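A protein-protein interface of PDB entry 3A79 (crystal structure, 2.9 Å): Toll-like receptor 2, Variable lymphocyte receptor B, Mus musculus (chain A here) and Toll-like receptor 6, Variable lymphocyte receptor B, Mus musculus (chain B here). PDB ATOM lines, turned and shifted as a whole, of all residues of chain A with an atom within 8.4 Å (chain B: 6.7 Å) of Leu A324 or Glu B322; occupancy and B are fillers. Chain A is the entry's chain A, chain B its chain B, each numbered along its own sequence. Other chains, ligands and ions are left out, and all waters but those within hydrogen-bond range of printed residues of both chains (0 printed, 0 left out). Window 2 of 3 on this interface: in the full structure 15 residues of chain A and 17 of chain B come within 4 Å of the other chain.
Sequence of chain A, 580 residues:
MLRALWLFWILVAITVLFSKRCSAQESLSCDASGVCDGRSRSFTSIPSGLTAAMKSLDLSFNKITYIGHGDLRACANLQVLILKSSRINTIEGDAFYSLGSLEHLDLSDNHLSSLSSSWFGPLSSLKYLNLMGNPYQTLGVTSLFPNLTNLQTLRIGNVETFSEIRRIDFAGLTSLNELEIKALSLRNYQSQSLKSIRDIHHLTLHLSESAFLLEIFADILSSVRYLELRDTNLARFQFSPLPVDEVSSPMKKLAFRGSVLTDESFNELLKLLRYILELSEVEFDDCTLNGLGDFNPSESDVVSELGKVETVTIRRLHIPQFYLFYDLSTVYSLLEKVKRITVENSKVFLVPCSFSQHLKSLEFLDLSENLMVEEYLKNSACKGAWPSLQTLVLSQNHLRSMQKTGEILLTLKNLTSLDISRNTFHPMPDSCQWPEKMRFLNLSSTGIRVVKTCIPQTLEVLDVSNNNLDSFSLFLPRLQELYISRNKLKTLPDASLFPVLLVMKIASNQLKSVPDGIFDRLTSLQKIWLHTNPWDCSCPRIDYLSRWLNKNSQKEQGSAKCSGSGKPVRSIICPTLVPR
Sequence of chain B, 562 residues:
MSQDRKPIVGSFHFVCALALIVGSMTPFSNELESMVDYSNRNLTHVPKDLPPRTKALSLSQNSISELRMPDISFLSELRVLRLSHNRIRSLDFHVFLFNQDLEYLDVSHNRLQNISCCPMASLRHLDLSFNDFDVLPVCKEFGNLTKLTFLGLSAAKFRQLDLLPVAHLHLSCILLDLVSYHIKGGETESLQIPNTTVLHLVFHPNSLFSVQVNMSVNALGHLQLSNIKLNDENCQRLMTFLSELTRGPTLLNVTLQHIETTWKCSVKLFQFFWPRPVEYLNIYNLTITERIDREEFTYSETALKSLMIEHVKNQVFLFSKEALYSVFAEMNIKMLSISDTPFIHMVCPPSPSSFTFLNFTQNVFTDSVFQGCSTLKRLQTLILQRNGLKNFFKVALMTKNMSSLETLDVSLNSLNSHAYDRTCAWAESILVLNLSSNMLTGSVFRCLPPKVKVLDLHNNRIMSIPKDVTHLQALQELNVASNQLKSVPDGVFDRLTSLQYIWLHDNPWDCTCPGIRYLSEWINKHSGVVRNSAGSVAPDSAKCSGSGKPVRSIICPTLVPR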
ATOM      1  N   ASP A 263      14.495  29.485 -20.772  1.00  0.00           N
ATOM      2  CA  ASP A 263      14.221  29.538 -22.196  1.00  0.00           C
ATOM      3  C   ASP A 263      13.052  30.471 -22.497  1.00  0.00           C
ATOM      4  O   ASP A 263      13.009  31.089 -23.547  1.00  0.00           O
ATOM      5  CB  ASP A 263      13.983  28.137 -22.742  1.00  0.00           C
ATOM      6  CG  ASP A 263      15.273  27.387 -22.974  1.00  0.00           C
ATOM      7  OD1 ASP A 263      15.259  26.133 -23.005  1.00  0.00           O
ATOM      8  OD2 ASP A 263      16.304  28.068 -23.133  1.00  0.00           O
ATOM      9  N   GLY A 291      17.795  26.161 -18.689  1.00  0.00           N
ATOM     10  CA  GLY A 291      17.129  25.945 -19.953  1.00  0.00           C
ATOM     11  C   GLY A 291      18.074  25.197 -20.871  1.00  0.00           C
ATOM     12  O   GLY A 291      19.116  24.714 -20.431  1.00  0.00           O
ATOM     13  N   LEU A 292      17.714  25.107 -22.146  1.00  0.00           N
ATOM     14  CA  LEU A 292      18.441  24.263 -23.078  1.00  0.00           C
ATOM     15  C   LEU A 292      18.349  24.843 -24.469  1.00  0.00           C
ATOM     16  O   LEU A 292      18.539  24.128 -25.450  1.00  0.00           O
ATOM     17  CB  LEU A 292      17.862  22.839 -23.102  1.00  0.00           C
ATOM     18  CG  LEU A 292      17.954  21.905 -21.893  1.00  0.00           C
ATOM     19  CD1 LEU A 292      17.246  20.609 -22.197  1.00  0.00           C
ATOM     20  CD2 LEU A 292      19.387  21.620 -21.515  1.00  0.00           C
ATOM     21  N   GLY A 293      18.032  26.129 -24.556  1.00  0.00           N
ATOM     22  CA  GLY A 293      17.968  26.804 -25.840  1.00  0.00           C
ATOM     23  C   GLY A 293      16.705  26.522 -26.636  1.00  0.00           C
ATOM     24  O   GLY A 293      16.679  26.722 -27.850  1.00  0.00           O
ATOM     25  N   ASP A 294      15.663  26.051 -25.951  1.00  0.00           N
ATOM     26  CA  ASP A 294      14.356  25.834 -26.569  1.00  0.00           C
ATOM     27  C   ASP A 294      13.605  27.165 -26.745  1.00  0.00           C
ATOM     28  O   ASP A 294      12.572  27.409 -26.107  1.00  0.00           O
ATOM     29  CB  ASP A 294      13.531  24.852 -25.729  1.00  0.00           C
ATOM     30  CG  ASP A 294      12.382  24.215 -26.514  1.00  0.00           C
ATOM     31  OD1 ASP A 294      11.412  23.724 -25.878  1.00  0.00           O
ATOM     32  OD2 ASP A 294      12.458  24.203 -27.764  1.00  0.00           O
ATOM     33  N   ILE A 319      25.099  26.817 -17.735  1.00  0.00           N
ATOM     34  CA  ILE A 319      23.967  26.073 -18.245  1.00  0.00           C
ATOM     35  C   ILE A 319      24.049  24.680 -17.646  1.00  0.00           C
ATOM     36  O   ILE A 319      24.795  23.836 -18.142  1.00  0.00           O
ATOM     37  CB  ILE A 319      24.039  26.005 -19.769  1.00  0.00           C
ATOM     38  CG1 ILE A 319      24.047  27.418 -20.341  1.00  0.00           C
ATOM     39  CG2 ILE A 319      22.883  25.227 -20.331  1.00  0.00           C
ATOM     40  CD1 ILE A 319      24.509  27.501 -21.772  1.00  0.00           C
ATOM     41  N   PRO A 320      23.280  24.445 -16.566  1.00  0.00           N
ATOM     42  CA  PRO A 320      23.319  23.234 -15.740  1.00  0.00           C
ATOM     43  C   PRO A 320      23.431  21.941 -16.532  1.00  0.00           C
ATOM     44  O   PRO A 320      24.273  21.105 -16.198  1.00  0.00           O
ATOM     45  CB  PRO A 320      21.989  23.284 -14.987  1.00  0.00           C
ATOM     46  CG  PRO A 320      21.672  24.723 -14.876  1.00  0.00           C
ATOM     47  CD  PRO A 320      22.224  25.375 -16.124  1.00  0.00           C
ATOM     48  N   GLN A 321      22.592  21.757 -17.544  1.00  0.00           N
ATOM     49  CA  GLN A 321      22.664  20.530 -18.328  1.00  0.00           C
ATOM     50  C   GLN A 321      23.165  20.862 -19.711  1.00  0.00           C
ATOM     51  O   GLN A 321      22.533  20.527 -20.708  1.00  0.00           O
ATOM     52  CB  GLN A 321      21.303  19.853 -18.424  1.00  0.00           C
ATOM     53  CG  GLN A 321      20.855  19.135 -17.173  1.00  0.00           C
ATOM     54  CD  GLN A 321      19.385  18.773 -17.232  1.00  0.00           C
ATOM     55  OE1 GLN A 321      18.546  19.612 -17.580  1.00  0.00           O
ATOM     56  NE2 GLN A 321      19.063  17.522 -16.895  1.00  0.00           N
ATOM     57  N   PHE A 322      24.316  21.522 -19.759  1.00  0.00           N
ATOM     58  CA  PHE A 322      24.854  22.054 -20.996  1.00  0.00           C
ATOM     59  C   PHE A 322      24.815  21.034 -22.142  1.00  0.00           C
ATOM     60  O   PHE A 322      24.561  21.409 -23.287  1.00  0.00           O
ATOM     61  CB  PHE A 322      26.269  22.566 -20.764  1.00  0.00           C
ATOM     62  CG  PHE A 322      27.315  21.495 -20.808  1.00  0.00           C
ATOM     63  CD1 PHE A 322      27.987  21.208 -21.987  1.00  0.00           C
ATOM     64  CD2 PHE A 322      27.623  20.768 -19.679  1.00  0.00           C
ATOM     65  CE1 PHE A 322      28.941  20.207 -22.032  1.00  0.00           C
ATOM     66  CE2 PHE A 322      28.582  19.768 -19.722  1.00  0.00           C
ATOM     67  CZ  PHE A 322      29.237  19.486 -20.895  1.00  0.00           C
ATOM     68  N   TYR A 323      25.041  19.755 -21.829  1.00  0.00           N
ATOM     69  CA  TYR A 323      25.152  18.695 -22.844  1.00  0.00           C
ATOM     70  C   TYR A 323      23.834  18.372 -23.551  1.00  0.00           C
ATOM     71  O   TYR A 323      23.824  17.736 -24.606  1.00  0.00           O
ATOM     72  CB  TYR A 323      25.768  17.414 -22.245  1.00  0.00           C
ATOM     73  CG  TYR A 323      24.881  16.721 -21.229  1.00  0.00           C
ATOM     74  CD1 TYR A 323      24.243  15.529 -21.530  1.00  0.00           C
ATOM     75  CD2 TYR A 323      24.672  17.270 -19.978  1.00  0.00           C
ATOM     76  CE1 TYR A 323      23.420  14.901 -20.601  1.00  0.00           C
ATOM     77  CE2 TYR A 323      23.858  16.665 -19.058  1.00  0.00           C
ATOM     78  CZ  TYR A 323      23.230  15.478 -19.368  1.00  0.00           C
ATOM     79  OH  TYR A 323      22.414  14.872 -18.432  1.00  0.00           O
ATOM     80  N   LEU A 324      22.724  18.820 -22.975  1.00  0.00           N
ATOM     81  CA  LEU A 324      21.408  18.525 -23.527  1.00  0.00           C
ATOM     82  C   LEU A 324      20.913  19.679 -24.375  1.00  0.00           C
ATOM     83  O   LEU A 324      19.741  19.764 -24.706  1.00  0.00           O
ATOM     84  CB  LEU A 324      20.413  18.269 -22.398  1.00  0.00           C
ATOM     85  CG  LEU A 324      20.634  17.053 -21.496  1.00  0.00           C
ATOM     86  CD1 LEU A 324      19.486  16.917 -20.518  1.00  0.00           C
ATOM     87  CD2 LEU A 324      20.791  15.786 -22.320  1.00  0.00           C
ATOM     88  N   PHE A 325      21.813  20.580 -24.723  1.00  0.00           N
ATOM     89  CA  PHE A 325      21.402  21.813 -25.377  1.00  0.00           C
ATOM     90  C   PHE A 325      20.833  21.552 -26.762  1.00  0.00           C
ATOM     91  O   PHE A 325      21.329  20.701 -27.499  1.00  0.00           O
ATOM     92  CB  PHE A 325      22.567  22.809 -25.443  1.00  0.00           C
ATOM     93  CG  PHE A 325      22.146  24.234 -25.264  1.00  0.00           C
ATOM     94  CD1 PHE A 325      21.966  24.760 -23.988  1.00  0.00           C
ATOM     95  CD2 PHE A 325      21.910  25.045 -26.361  1.00  0.00           C
ATOM     96  CE1 PHE A 325      21.571  26.058 -23.809  1.00  0.00           C
ATOM     97  CE2 PHE A 325      21.511  26.354 -26.188  1.00  0.00           C
ATOM     98  CZ  PHE A 325      21.340  26.860 -24.912  1.00  0.00           C
ATOM     99  N   TYR A 326      19.789  22.295 -27.106  1.00  0.00           N
ATOM    100  CA  TYR A 326      19.111  22.120 -28.380  1.00  0.00           C
ATOM    101  C   TYR A 326      19.870  22.680 -29.589  1.00  0.00           C
ATOM    102  O   TYR A 326      20.911  23.333 -29.467  1.00  0.00           O
ATOM    103  CB  TYR A 326      17.698  22.712 -28.342  1.00  0.00           C
ATOM    104  CG  TYR A 326      16.687  21.888 -27.569  1.00  0.00           C
ATOM    105  CD1 TYR A 326      16.326  22.234 -26.280  1.00  0.00           C
ATOM    106  CD2 TYR A 326      16.087  20.770 -28.131  1.00  0.00           C
ATOM    107  CE1 TYR A 326      15.407  21.490 -25.568  1.00  0.00           C
ATOM    108  CE2 TYR A 326      15.160  20.022 -27.422  1.00  0.00           C
ATOM    109  CZ  TYR A 326      14.825  20.395 -26.141  1.00  0.00           C
ATOM    110  OH  TYR A 326      13.906  19.684 -25.406  1.00  0.00           O
ATOM    111  N   ASP A 327      19.298  22.389 -30.755  1.00  0.00           N
ATOM    112  CA  ASP A 327      19.786  22.763 -32.077  1.00  0.00           C
ATOM    113  C   ASP A 327      20.125  24.237 -32.177  1.00  0.00           C
ATOM    114  O   ASP A 327      20.989  24.646 -32.970  1.00  0.00           O
ATOM    115  CB  ASP A 327      18.668  22.476 -33.069  1.00  0.00           C
ATOM    116  CG  ASP A 327      19.173  22.269 -34.448  1.00  0.00           C
ATOM    117  OD1 ASP A 327      20.347  22.615 -34.691  1.00  0.00           O
ATOM    118  OD2 ASP A 327      18.403  21.749 -35.283  1.00  0.00           O
ATOM    119  N   PHE A 349      30.440  23.293 -27.285  1.00  0.00           N
ATOM    120  CA  PHE A 349      31.111  22.114 -27.820  1.00  0.00           C
ATOM    121  C   PHE A 349      30.784  21.864 -29.273  1.00  0.00           C
ATOM    122  O   PHE A 349      31.333  20.950 -29.873  1.00  0.00           O
ATOM    123  CB  PHE A 349      30.776  20.867 -27.012  1.00  0.00           C
ATOM    124  CG  PHE A 349      29.323  20.504 -27.038  1.00  0.00           C
ATOM    125  CD1 PHE A 349      28.791  19.783 -28.102  1.00  0.00           C
ATOM    126  CD2 PHE A 349      28.486  20.878 -25.997  1.00  0.00           C
ATOM    127  CE1 PHE A 349      27.443  19.437 -28.132  1.00  0.00           C
ATOM    128  CE2 PHE A 349      27.140  20.541 -26.014  1.00  0.00           C
ATOM    129  CZ  PHE A 349      26.616  19.816 -27.087  1.00  0.00           C
ATOM    130  N   ARG B 294      16.767   6.907 -29.663  1.00  0.00           N
ATOM    131  CA  ARG B 294      16.523   6.170 -28.429  1.00  0.00           C
ATOM    132  C   ARG B 294      16.293   4.706 -28.767  1.00  0.00           C
ATOM    133  O   ARG B 294      15.338   4.366 -29.466  1.00  0.00           O
ATOM    134  CB  ARG B 294      15.332   6.742 -27.653  1.00  0.00           C
ATOM    135  CG  ARG B 294      15.722   7.582 -26.445  1.00  0.00           C
ATOM    136  CD  ARG B 294      14.506   8.239 -25.782  1.00  0.00           C
ATOM    137  NE  ARG B 294      14.123   9.509 -26.406  1.00  0.00           N
ATOM    138  CZ  ARG B 294      14.636  10.692 -26.072  1.00  0.00           C
ATOM    139  NH1 ARG B 294      15.560  10.765 -25.118  1.00  0.00           N
ATOM    140  NH2 ARG B 294      14.231  11.798 -26.688  1.00  0.00           N
ATOM    141  N   PHE B 297      16.541  -1.269 -24.712  1.00  0.00           N
ATOM    142  CA  PHE B 297      17.533  -2.111 -24.062  1.00  0.00           C
ATOM    143  C   PHE B 297      17.195  -2.308 -22.590  1.00  0.00           C
ATOM    144  O   PHE B 297      16.671  -1.407 -21.937  1.00  0.00           O
ATOM    145  CB  PHE B 297      18.939  -1.518 -24.211  1.00  0.00           C
ATOM    146  CG  PHE B 297      19.108  -0.184 -23.546  1.00  0.00           C
ATOM    147  CD1 PHE B 297      19.682  -0.090 -22.287  1.00  0.00           C
ATOM    148  CD2 PHE B 297      18.680   0.980 -24.179  1.00  0.00           C
ATOM    149  CE1 PHE B 297      19.828   1.146 -21.671  1.00  0.00           C
ATOM    150  CE2 PHE B 297      18.820   2.209 -23.577  1.00  0.00           C
ATOM    151  CZ  PHE B 297      19.399   2.297 -22.321  1.00  0.00           C
ATOM    152  N   PHE B 319      21.668  14.877 -32.075  1.00  0.00           N
ATOM    153  CA  PHE B 319      20.969  13.752 -31.482  1.00  0.00           C
ATOM    154  C   PHE B 319      20.780  13.984 -29.998  1.00  0.00           C
ATOM    155  O   PHE B 319      21.514  14.753 -29.399  1.00  0.00           O
ATOM    156  CB  PHE B 319      21.762  12.476 -31.704  1.00  0.00           C
ATOM    157  CG  PHE B 319      23.101  12.481 -31.058  1.00  0.00           C
ATOM    158  CD1 PHE B 319      23.265  11.987 -29.771  1.00  0.00           C
ATOM    159  CD2 PHE B 319      24.210  12.960 -31.738  1.00  0.00           C
ATOM    160  CE1 PHE B 319      24.525  11.976 -29.165  1.00  0.00           C
ATOM    161  CE2 PHE B 319      25.468  12.949 -31.142  1.00  0.00           C
ATOM    162  CZ  PHE B 319      25.626  12.456 -29.852  1.00  0.00           C
ATOM    163  N   SER B 320      19.802  13.326 -29.393  1.00  0.00           N
ATOM    164  CA  SER B 320      19.631  13.485 -27.958  1.00  0.00           C
ATOM    165  C   SER B 320      20.737  12.754 -27.204  1.00  0.00           C
ATOM    166  O   SER B 320      20.835  11.533 -27.268  1.00  0.00           O
ATOM    167  CB  SER B 320      18.269  12.982 -27.500  1.00  0.00           C
ATOM    168  OG  SER B 320      18.209  12.983 -26.084  1.00  0.00           O
ATOM    169  N   LYS B 321      21.568  13.499 -26.484  1.00  0.00           N
ATOM    170  CA  LYS B 321      22.707  12.889 -25.809  1.00  0.00           C
ATOM    171  C   LYS B 321      22.293  11.841 -24.762  1.00  0.00           C
ATOM    172  O   LYS B 321      23.069  10.930 -24.452  1.00  0.00           O
ATOM    173  CB  LYS B 321      23.644  13.952 -25.220  1.00  0.00           C
ATOM    174  CG  LYS B 321      24.440  14.738 -26.262  1.00  0.00           C
ATOM    175  CD  LYS B 321      23.529  15.685 -27.047  1.00  0.00           C
ATOM    176  CE  LYS B 321      24.240  16.264 -28.252  1.00  0.00           C
ATOM    177  NZ  LYS B 321      25.328  15.349 -28.659  1.00  0.00           N
ATOM    178  N   GLU B 322      21.075  11.956 -24.231  1.00  0.00           N
ATOM    179  CA  GLU B 322      20.537  10.909 -23.361  1.00  0.00           C
ATOM    180  C   GLU B 322      20.582   9.567 -24.088  1.00  0.00           C
ATOM    181  O   GLU B 322      21.103   8.581 -23.565  1.00  0.00           O
ATOM    182  CB  GLU B 322      19.104  11.226 -22.937  1.00  0.00           C
ATOM    183  CG  GLU B 322      18.997  12.160 -21.746  1.00  0.00           C
ATOM    184  CD  GLU B 322      17.857  13.173 -21.883  1.00  0.00           C
ATOM    185  OE1 GLU B 322      17.187  13.458 -20.863  1.00  0.00           O
ATOM    186  OE2 GLU B 322      17.635  13.691 -23.008  1.00  0.00           O
ATOM    187  N   ALA B 323      20.055   9.563 -25.313  1.00  0.00           N
ATOM    188  CA  ALA B 323      19.912   8.355 -26.129  1.00  0.00           C
ATOM    189  C   ALA B 323      21.205   7.579 -26.264  1.00  0.00           C
ATOM    190  O   ALA B 323      21.190   6.359 -26.447  1.00  0.00           O
ATOM    191  CB  ALA B 323      19.371   8.707 -27.505  1.00  0.00           C
ATOM    192  N   LEU B 324      22.318   8.298 -26.181  1.00  0.00           N
ATOM    193  CA  LEU B 324      23.638   7.707 -26.311  1.00  0.00           C
ATOM    194  C   LEU B 324      24.220   7.391 -24.938  1.00  0.00           C
ATOM    195  O   LEU B 324      24.623   6.261 -24.699  1.00  0.00           O
ATOM    196  CB  LEU B 324      24.564   8.636 -27.110  1.00  0.00           C
ATOM    197  CG  LEU B 324      26.082   8.401 -27.065  1.00  0.00           C
ATOM    198  CD1 LEU B 324      26.495   7.193 -27.887  1.00  0.00           C
ATOM    199  CD2 LEU B 324      26.810   9.622 -27.554  1.00  0.00           C
ATOM    200  N   TYR B 325      24.250   8.367 -24.030  1.00  0.00           N
ATOM    201  CA  TYR B 325      24.937   8.168 -22.746  1.00  0.00           C
ATOM    202  C   TYR B 325      24.231   7.205 -21.779  1.00  0.00           C
ATOM    203  O   TYR B 325      24.876   6.543 -20.960  1.00  0.00           O
ATOM    204  CB  TYR B 325      25.242   9.497 -22.033  1.00  0.00           C
ATOM    205  CG  TYR B 325      26.167  10.425 -22.792  1.00  0.00           C
ATOM    206  CD1 TYR B 325      25.923  11.791 -22.838  1.00  0.00           C
ATOM    207  CD2 TYR B 325      27.278   9.940 -23.466  1.00  0.00           C
ATOM    208  CE1 TYR B 325      26.754  12.645 -23.531  1.00  0.00           C
ATOM    209  CE2 TYR B 325      28.121  10.791 -24.164  1.00  0.00           C
ATOM    210  CZ  TYR B 325      27.851  12.146 -24.193  1.00  0.00           C
ATOM    211  OH  TYR B 325      28.673  13.006 -24.892  1.00  0.00           O
ATOM    212  N   SER B 326      22.912   7.116 -21.861  1.00  0.00           N
ATOM    213  CA  SER B 326      22.199   6.263 -20.917  1.00  0.00           C
ATOM    214  C   SER B 326      22.491   4.776 -21.179  1.00  0.00           C
ATOM    215  O   SER B 326      22.596   3.979 -20.247  1.00  0.00           O
ATOM    216  CB  SER B 326      20.706   6.562 -20.944  1.00  0.00           C
ATOM    217  OG  SER B 326      20.206   6.334 -22.245  1.00  0.00           O
ATOM    218  N   VAL B 327      22.638   4.422 -22.451  1.00  0.00           N
ATOM    219  CA  VAL B 327      23.016   3.069 -22.855  1.00  0.00           C
ATOM    220  C   VAL B 327      24.239   2.538 -22.099  1.00  0.00           C
ATOM    221  O   VAL B 327      24.359   1.334 -21.886  1.00  0.00           O
ATOM    222  CB  VAL B 327      23.269   3.017 -24.371  1.00  0.00           C
ATOM    223  CG1 VAL B 327      24.026   1.760 -24.765  1.00  0.00           C
ATOM    224  CG2 VAL B 327      21.949   3.130 -25.118  1.00  0.00           C
ATOM    225  N   ILE B 344      31.327  14.553 -24.282  1.00  0.00           N
ATOM    226  CA  ILE B 344      31.406  15.775 -23.485  1.00  0.00           C
ATOM    227  C   ILE B 344      30.922  15.573 -22.049  1.00  0.00           C
ATOM    228  O   ILE B 344      30.964  16.501 -21.231  1.00  0.00           O
ATOM    229  CB  ILE B 344      30.558  16.884 -24.109  1.00  0.00           C
ATOM    230  CG1 ILE B 344      29.113  16.421 -24.236  1.00  0.00           C
ATOM    231  CG2 ILE B 344      31.084  17.264 -25.470  1.00  0.00           C
ATOM    232  CD1 ILE B 344      28.191  17.478 -24.814  1.00  0.00           C
ATOM    233  N   VAL B 347      26.227  10.553 -18.030  1.00  0.00           N
ATOM    234  CA  VAL B 347      25.023  10.679 -17.223  1.00  0.00           C
ATOM    235  C   VAL B 347      25.188   9.949 -15.893  1.00  0.00           C
ATOM    236  O   VAL B 347      25.915   8.967 -15.810  1.00  0.00           O
ATOM    237  CB  VAL B 347      23.809  10.127 -18.001  1.00  0.00           C
ATOM    238  CG1 VAL B 347      22.695   9.750 -17.074  1.00  0.00           C
ATOM    239  CG2 VAL B 347      23.334  11.150 -19.007  1.00  0.00           C
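OE2 of Glu B322 lies within hydrogen-bond range of OG of Ser B320.
The side-chain hydroxyl (OG) of Ser B326 sits at hydrogen-bond distance from the backbone carbonyl oxygen (O) of Glu B322 (2.8 Å).
The side-chain hydroxyl (OH) of Tyr B325 lies within hydrogen-bond range of the backbone NH (N) of Ile B344, 3.1 Å away.
Among the printed residues, pairs that only touch across the chains: Tyr A323 with Lys B321, Phe A349 with Ile B344, Phe A322 with Ile B344, Tyr A323 with Ile B344, Leu A324 with Glu B322 and Tyr A323 with Val B347.
Ile A319 touches none of the printed residues of chain B.
Pro A320 touches none of the printed residues of chain B.
Of chain B, only Glu B322 comes within 4 Å of Leu A324.
Of the printed residues of chain A, Lys B321 touches Tyr A323.
Glu B322 touches one residue of chain A.
Printed residues of chain A within 4 Å of Val B347: Tyr A323 (3.9 Å).
The nearest residue of chain A that does not touch Glu B322 is Tyr A323 (5.2 Å).
The nearest printed residue of chain A that does not touch Ile B344 is Leu A324 (5.9 Å).
Printed residues of chain A that touch a printed residue of chain B: Phe A322, Tyr A323, Leu A324 and Phe A349.
Of the 13 printed residues of chain B, 4 touch a printed residue of chain A.
Hydrophobic or aromatic side chains of chain B that line the printed part of chain A: Ile B344 and Val B347.
Among the printed residues, 6 pairs touch across the chains.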
